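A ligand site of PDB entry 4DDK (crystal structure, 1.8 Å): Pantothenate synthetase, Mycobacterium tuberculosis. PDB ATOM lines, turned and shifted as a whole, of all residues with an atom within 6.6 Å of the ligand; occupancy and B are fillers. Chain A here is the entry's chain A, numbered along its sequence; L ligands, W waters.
N of Val 187 sits at hydrogen-bond distance from O4 of the ligand (3.0 Å).
NE2 of His 44 lies within hydrogen-bond range of O2 of the ligand, 3.0 Å away.
A ring nitrogen (NE2) of His 47 is in hydrogen-bond range of an oxygen (O1) of the ligand (3.3 Å).
The backbone carbonyl oxygen of Val 187 lies within hydrogen-bond range of the backbone NH of Met 195, at 3.0 Å.
A ring nitrogen (ND1) of His 47 lies within hydrogen-bond range of the backbone NH of His 44 (3.0 Å).
ND1 of His 44 is in hydrogen-bond range of N of Gly 46, at 2.9 Å.
The side-chain sulfur (SD) of Met 195 lies within hydrogen-bond range of the backbone NH (N) of Gly 46.
The side-chain hydroxyl (OG1) of Thr 186 sits at hydrogen-bond distance from the backbone NH (N) of Lys 160, 3.1 Å away.
The backbone carbonyl oxygen of Phe 157 lies within hydrogen-bond range of the backbone NH of Val 184 (2.9 Å).
The backbone carbonyl oxygen (O) of Val 184 lies within hydrogen-bond range of the backbone NH (N) of Glu 159, at 2.9 Å.
O of Gly 46 lies close to O3 of the ligand, 3.5 Å away.
Leu 50 touches the ligand (CD2 to O3, 3.5 Å).
Gly 158 touches the ligand (CA to O3, 3.2 Å).
CG of Lys 160 touches C8 of the ligand (3.8 Å).
O of Val 184 touches C5 of the ligand, 3.6 Å away.
O of Pro 185 touches C5 of the ligand, at 3.3 Å.
Thr 186 touches the ligand (CA to O4, 3.4 Å).
Met 195 touches the ligand.
Ser 196 touches the ligand (CA to O2, 3.96 Å).
Hydrophobic or aromatic side chains within 4 Å of the ligand: His 44, His 47, Leu 50, Val 184 and Val 187.
Of the 22 residues printed, 12 come within 4 Å of the ligand.
The nearest printed residue that does not touch the ligand is Asp 161 (4.3 Å).
Water W1 lies within hydrogen-bond range of the side-chain carboxylate of Asp 161 (2.6 Å) and an oxygen (O1) of the ligand (3.0 Å).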
ATOM      1  N   HIS A  44      31.917  18.052 -16.671  1.00  0.00           N
ATOM      2  CA  HIS A  44      32.261  16.833 -15.918  1.00  0.00           C
ATOM      3  C   HIS A  44      32.138  15.603 -16.830  1.00  0.00           C
ATOM      4  O   HIS A  44      31.915  15.713 -18.034  1.00  0.00           O
ATOM      5  CB  HIS A  44      31.292  16.708 -14.752  1.00  0.00           C
ATOM      6  CG  HIS A  44      29.859  16.813 -15.157  1.00  0.00           C
ATOM      7  ND1 HIS A  44      29.268  15.923 -16.018  1.00  0.00           N
ATOM      8  CD2 HIS A  44      28.924  17.753 -14.893  1.00  0.00           C
ATOM      9  CE1 HIS A  44      28.011  16.278 -16.244  1.00  0.00           C
ATOM     10  NE2 HIS A  44      27.773  17.376 -15.557  1.00  0.00           N
ATOM     11  N   GLU A  45      32.224  14.413 -16.258  1.00  0.00           N
ATOM     12  CA  GLU A  45      32.226  13.180 -17.034  1.00  0.00           C
ATOM     13  C   GLU A  45      30.961  12.937 -17.891  1.00  0.00           C
ATOM     14  O   GLU A  45      31.028  12.309 -18.964  1.00  0.00           O
ATOM     15  CB  GLU A  45      32.441  12.019 -16.058  1.00  0.00           C
ATOM     16  CG  GLU A  45      32.360  10.648 -16.701  1.00  0.00           C
ATOM     17  CD  GLU A  45      33.582  10.344 -17.536  1.00  0.00           C
ATOM     18  OE1 GLU A  45      34.645  10.991 -17.370  1.00  0.00           O
ATOM     19  OE2 GLU A  45      33.447   9.456 -18.394  1.00  0.00           O
ATOM     20  N   GLY A  46      29.814  13.386 -17.420  1.00  0.00           N
ATOM     21  CA  GLY A  46      28.591  13.303 -18.239  1.00  0.00           C
ATOM     22  C   GLY A  46      28.673  14.099 -19.536  1.00  0.00           C
ATOM     23  O   GLY A  46      28.137  13.676 -20.564  1.00  0.00           O
ATOM     24  N   HIS A  47      29.329  15.255 -19.494  1.00  0.00           N
ATOM     25  CA  HIS A  47      29.616  16.015 -20.721  1.00  0.00           C
ATOM     26  C   HIS A  47      30.517  15.208 -21.632  1.00  0.00           C
ATOM     27  O   HIS A  47      30.311  15.156 -22.849  1.00  0.00           O
ATOM     28  CB  HIS A  47      30.223  17.402 -20.425  1.00  0.00           C
ATOM     29  CG  HIS A  47      29.310  18.321 -19.670  1.00  0.00           C
ATOM     30  ND1 HIS A  47      29.536  18.676 -18.351  1.00  0.00           N
ATOM     31  CD2 HIS A  47      28.150  18.932 -20.024  1.00  0.00           C
ATOM     32  CE1 HIS A  47      28.587  19.485 -17.939  1.00  0.00           C
ATOM     33  NE2 HIS A  47      27.727  19.654 -18.928  1.00  0.00           N
ATOM     34  N   ALA A  49      30.708  12.014 -21.919  1.00  0.00           N
ATOM     35  CA  ALA A  49      29.842  11.013 -22.583  1.00  0.00           C
ATOM     36  C   ALA A  49      29.096  11.569 -23.801  1.00  0.00           C
ATOM     37  O   ALA A  49      28.911  10.866 -24.813  1.00  0.00           O
ATOM     38  CB  ALA A  49      28.853  10.444 -21.579  1.00  0.00           C
ATOM     39  N   LEU A  50      28.606  12.802 -23.693  1.00  0.00           N
ATOM     40  CA  LEU A  50      28.059  13.526 -24.835  1.00  0.00           C
ATOM     41  C   LEU A  50      29.110  13.660 -25.939  1.00  0.00           C
ATOM     42  O   LEU A  50      28.846  13.398 -27.084  1.00  0.00           O
ATOM     43  CB  LEU A  50      27.594  14.948 -24.423  1.00  0.00           C
ATOM     44  CG  LEU A  50      26.462  15.057 -23.419  1.00  0.00           C
ATOM     45  CD1 LEU A  50      26.273  16.523 -23.047  1.00  0.00           C
ATOM     46  CD2 LEU A  50      25.173  14.460 -24.006  1.00  0.00           C
ATOM     47  N   TYR A  82      26.946  30.857 -11.238  1.00  0.00           N
ATOM     48  CA  TYR A  82      27.225  29.690 -12.098  1.00  0.00           C
ATOM     49  C   TYR A  82      28.713  29.364 -12.131  1.00  0.00           C
ATOM     50  O   TYR A  82      29.529  30.285 -12.312  1.00  0.00           O
ATOM     51  CB  TYR A  82      26.680  29.865 -13.529  1.00  0.00           C
ATOM     52  CG  TYR A  82      26.414  28.521 -14.153  1.00  0.00           C
ATOM     53  CD1 TYR A  82      25.222  27.814 -13.861  1.00  0.00           C
ATOM     54  CD2 TYR A  82      27.369  27.910 -14.960  1.00  0.00           C
ATOM     55  CE1 TYR A  82      25.005  26.514 -14.391  1.00  0.00           C
ATOM     56  CE2 TYR A  82      27.156  26.633 -15.488  1.00  0.00           C
ATOM     57  CZ  TYR A  82      25.972  25.946 -15.204  1.00  0.00           C
ATOM     58  OH  TYR A  82      25.775  24.687 -15.725  1.00  0.00           O
ATOM     59  N   PHE A 157      22.221  16.166 -26.309  1.00  0.00           N
ATOM     60  CA  PHE A 157      21.846  16.605 -24.980  1.00  0.00           C
ATOM     61  C   PHE A 157      21.744  15.428 -24.010  1.00  0.00           C
ATOM     62  O   PHE A 157      21.480  14.315 -24.446  1.00  0.00           O
ATOM     63  CB  PHE A 157      20.503  17.303 -25.081  1.00  0.00           C
ATOM     64  CG  PHE A 157      20.589  18.651 -25.727  1.00  0.00           C
ATOM     65  CD1 PHE A 157      20.226  18.829 -27.067  1.00  0.00           C
ATOM     66  CD2 PHE A 157      21.043  19.766 -24.983  1.00  0.00           C
ATOM     67  CE1 PHE A 157      20.302  20.093 -27.654  1.00  0.00           C
ATOM     68  CE2 PHE A 157      21.173  21.037 -25.593  1.00  0.00           C
ATOM     69  CZ  PHE A 157      20.777  21.204 -26.902  1.00  0.00           C
ATOM     70  N   GLY A 158      21.967  15.677 -22.722  1.00  0.00           N
ATOM     71  CA  GLY A 158      21.797  14.654 -21.671  1.00  0.00           C
ATOM     72  C   GLY A 158      20.326  14.476 -21.277  1.00  0.00           C
ATOM     73  O   GLY A 158      19.546  15.424 -21.360  1.00  0.00           O
ATOM     74  N   GLU A 159      19.959  13.276 -20.839  1.00  0.00           N
ATOM     75  CA  GLU A 159      18.640  12.999 -20.349  1.00  0.00           C
ATOM     76  C   GLU A 159      18.473  13.572 -18.949  1.00  0.00           C
ATOM     77  O   GLU A 159      17.358  13.639 -18.463  1.00  0.00           O
ATOM     78  CB  GLU A 159      18.363  11.493 -20.324  1.00  0.00           C
ATOM     79  CG  GLU A 159      18.078  10.919 -21.682  1.00  0.00           C
ATOM     80  CD  GLU A 159      17.834   9.411 -21.670  1.00  0.00           C
ATOM     81  OE1 GLU A 159      17.733   8.826 -20.555  1.00  0.00           O
ATOM     82  OE2 GLU A 159      17.763   8.830 -22.789  1.00  0.00           O
ATOM     83  N   LYS A 160      19.572  13.984 -18.337  1.00  0.00           N
ATOM     84  CA  LYS A 160      19.583  14.588 -16.995  1.00  0.00           C
ATOM     85  C   LYS A 160      18.581  15.753 -16.829  1.00  0.00           C
ATOM     86  O   LYS A 160      17.761  15.789 -15.926  1.00  0.00           O
ATOM     87  CB  LYS A 160      20.993  15.097 -16.733  1.00  0.00           C
ATOM     88  CG  LYS A 160      21.510  14.903 -15.356  1.00  0.00           C
ATOM     89  CD  LYS A 160      20.921  15.904 -14.466  1.00  0.00           C
ATOM     90  CE  LYS A 160      21.794  16.096 -13.278  1.00  0.00           C
ATOM     91  NZ  LYS A 160      21.049  16.993 -12.368  1.00  0.00           N
ATOM     92  N   ASP A 161      18.722  16.737 -17.699  1.00  0.00           N
ATOM     93  CA  ASP A 161      17.823  17.846 -17.786  1.00  0.00           C
ATOM     94  C   ASP A 161      16.798  17.399 -18.828  1.00  0.00           C
ATOM     95  O   ASP A 161      16.799  17.820 -19.994  1.00  0.00           O
ATOM     96  CB  ASP A 161      18.586  19.103 -18.182  1.00  0.00           C
ATOM     97  CG  ASP A 161      19.429  19.641 -17.038  1.00  0.00           C
ATOM     98  OD1 ASP A 161      18.924  19.749 -15.928  1.00  0.00           O
ATOM     99  OD2 ASP A 161      20.594  19.962 -17.260  1.00  0.00           O
ATOM    100  N   GLN A 164      14.231  19.875 -20.449  1.00  0.00           N
ATOM    101  CA  GLN A 164      14.920  20.633 -21.459  1.00  0.00           C
ATOM    102  C   GLN A 164      15.065  19.821 -22.766  1.00  0.00           C
ATOM    103  O   GLN A 164      14.898  20.374 -23.844  1.00  0.00           O
ATOM    104  CB  GLN A 164      16.273  21.070 -20.917  1.00  0.00           C
ATOM    105  CG  GLN A 164      17.236  21.688 -21.951  1.00  0.00           C
ATOM    106  CD  GLN A 164      18.556  21.994 -21.346  1.00  0.00           C
ATOM    107  OE1 GLN A 164      18.733  23.029 -20.704  1.00  0.00           O
ATOM    108  NE2 GLN A 164      19.492  21.072 -21.505  1.00  0.00           N
ATOM    109  N   VAL A 184      21.260  11.469 -24.591  1.00  0.00           N
ATOM    110  CA  VAL A 184      22.276  10.579 -24.032  1.00  0.00           C
ATOM    111  C   VAL A 184      21.981  10.276 -22.543  1.00  0.00           C
ATOM    112  O   VAL A 184      21.748  11.242 -21.760  1.00  0.00           O
ATOM    113  CB  VAL A 184      23.704  11.225 -24.156  1.00  0.00           C
ATOM    114  CG1 VAL A 184      24.823  10.299 -23.542  1.00  0.00           C
ATOM    115  CG2 VAL A 184      24.014  11.541 -25.624  1.00  0.00           C
ATOM    116  N   PRO A 185      21.888   8.959 -22.173  1.00  0.00           N
ATOM    117  CA  PRO A 185      21.621   8.529 -20.811  1.00  0.00           C
ATOM    118  C   PRO A 185      22.561   9.199 -19.816  1.00  0.00           C
ATOM    119  O   PRO A 185      23.746   9.346 -20.054  1.00  0.00           O
ATOM    120  CB  PRO A 185      21.867   6.998 -20.855  1.00  0.00           C
ATOM    121  CG  PRO A 185      21.601   6.612 -22.272  1.00  0.00           C
ATOM    122  CD  PRO A 185      21.990   7.807 -23.109  1.00  0.00           C
ATOM    123  N   THR A 186      21.977   9.606 -18.694  1.00  0.00           N
ATOM    124  CA  THR A 186      22.630  10.298 -17.614  1.00  0.00           C
ATOM    125  C   THR A 186      23.771   9.482 -17.034  1.00  0.00           C
ATOM    126  O   THR A 186      23.573   8.297 -16.708  1.00  0.00           O
ATOM    127  CB  THR A 186      21.581  10.545 -16.538  1.00  0.00           C
ATOM    128  OG1 THR A 186      20.492  11.281 -17.135  1.00  0.00           O
ATOM    129  CG2 THR A 186      22.147  11.265 -15.334  1.00  0.00           C
ATOM    130  N   VAL A 187      24.936  10.115 -16.903  1.00  0.00           N
ATOM    131  CA  VAL A 187      26.107   9.498 -16.204  1.00  0.00           C
ATOM    132  C   VAL A 187      25.945   9.725 -14.733  1.00  0.00           C
ATOM    133  O   VAL A 187      25.518  10.817 -14.295  1.00  0.00           O
ATOM    134  CB  VAL A 187      27.456  10.117 -16.652  1.00  0.00           C
ATOM    135  CG1 VAL A 187      28.651   9.354 -16.027  1.00  0.00           C
ATOM    136  CG2 VAL A 187      27.537  10.083 -18.143  1.00  0.00           C
ATOM    137  N   ARG A 188      26.283   8.692 -13.943  1.00  0.00           N
ATOM    138  CA  ARG A 188      26.073   8.720 -12.472  1.00  0.00           C
ATOM    139  C   ARG A 188      27.362   8.418 -11.719  1.00  0.00           C
ATOM    140  O   ARG A 188      28.202   7.694 -12.221  1.00  0.00           O
ATOM    141  CB  ARG A 188      25.000   7.700 -12.096  1.00  0.00           C
ATOM    142  CG  ARG A 188      23.659   8.050 -12.715  1.00  0.00           C
ATOM    143  CD  ARG A 188      22.564   7.058 -12.368  1.00  0.00           C
ATOM    144  NE  ARG A 188      21.305   7.476 -13.009  1.00  0.00           N
ATOM    145  CZ  ARG A 188      20.420   8.318 -12.460  1.00  0.00           C
ATOM    146  NH1 ARG A 188      20.642   8.823 -11.268  1.00  0.00           N
ATOM    147  NH2 ARG A 188      19.304   8.654 -13.105  1.00  0.00           N
ATOM    148  N   ALA A 194      23.187  11.430  -9.918  1.00  0.00           N
ATOM    149  CA  ALA A 194      23.333  12.053 -11.242  1.00  0.00           C
ATOM    150  C   ALA A 194      24.463  13.099 -11.220  1.00  0.00           C
ATOM    151  O   ALA A 194      24.497  13.987 -10.378  1.00  0.00           O
ATOM    152  CB  ALA A 194      22.047  12.694 -11.699  1.00  0.00           C
ATOM    153  N   MET A 195      25.369  12.985 -12.168  1.00  0.00           N
ATOM    154  CA  MET A 195      26.378  14.009 -12.336  1.00  0.00           C
ATOM    155  C   MET A 195      25.770  15.362 -12.721  1.00  0.00           C
ATOM    156  O   MET A 195      24.767  15.448 -13.471  1.00  0.00           O
ATOM    157  CB  MET A 195      27.418  13.563 -13.333  1.00  0.00           C
ATOM    158  CG  MET A 195      28.471  12.690 -12.638  1.00  0.00           C
ATOM    159  SD  MET A 195      29.651  12.221 -13.837  1.00  0.00           S
ATOM    160  CE  MET A 195      30.547  10.993 -12.881  1.00  0.00           C
ATOM    161  N   SER A 196      26.385  16.417 -12.191  1.00  0.00           N
ATOM    162  CA  SER A 196      25.926  17.789 -12.422  1.00  0.00           C
ATOM    163  C   SER A 196      27.032  18.734 -12.032  1.00  0.00           C
ATOM    164  O   SER A 196      27.773  18.443 -11.096  1.00  0.00           O
ATOM    165  CB  SER A 196      24.736  18.073 -11.502  1.00  0.00           C
ATOM    166  OG  SER A 196      24.406  19.448 -11.497  1.00  0.00           O
ATOM    167  N   SER A 197      27.084  19.891 -12.711  1.00  0.00           N
ATOM    168  CA  SER A 197      27.988  20.984 -12.304  1.00  0.00           C
ATOM    169  C   SER A 197      27.551  21.574 -10.925  1.00  0.00           C
ATOM    170  O   SER A 197      28.295  22.333 -10.259  1.00  0.00           O
ATOM    171  CB  SER A 197      28.019  22.062 -13.405  1.00  0.00           C
ATOM    172  OG  SER A 197      28.497  21.526 -14.663  1.00  0.00           O
HETATM  173  O1  LIG L   1      24.591  18.726 -18.276  1.00  0.00           O
HETATM  174  C1  LIG L   1      24.749  17.818 -17.431  1.00  0.00           C
HETATM  175  O2  LIG L   1      24.915  18.196 -16.229  1.00  0.00           O
HETATM  176  C2  LIG L   1      24.802  16.441 -17.789  1.00  0.00           C
HETATM  177  C3  LIG L   1      24.699  15.949 -19.103  1.00  0.00           C
HETATM  178  C4  LIG L   1      24.773  14.600 -19.366  1.00  0.00           C
HETATM  179  O3  LIG L   1      24.677  13.958 -20.576  1.00  0.00           O
HETATM  180  C5  LIG L   1      24.752  12.509 -20.295  1.00  0.00           C
HETATM  181  O4  LIG L   1      25.049  12.371 -18.854  1.00  0.00           O
HETATM  182  C6  LIG L   1      24.959  13.685 -18.364  1.00  0.00           C
HETATM  183  C7  LIG L   1      25.083  14.112 -17.093  1.00  0.00           C
HETATM  184  C8  LIG L   1      25.009  15.476 -16.781  1.00  0.00           C
HETATM  185  O   HOH W   1      21.951  19.375 -19.445  1.00  0.00           O
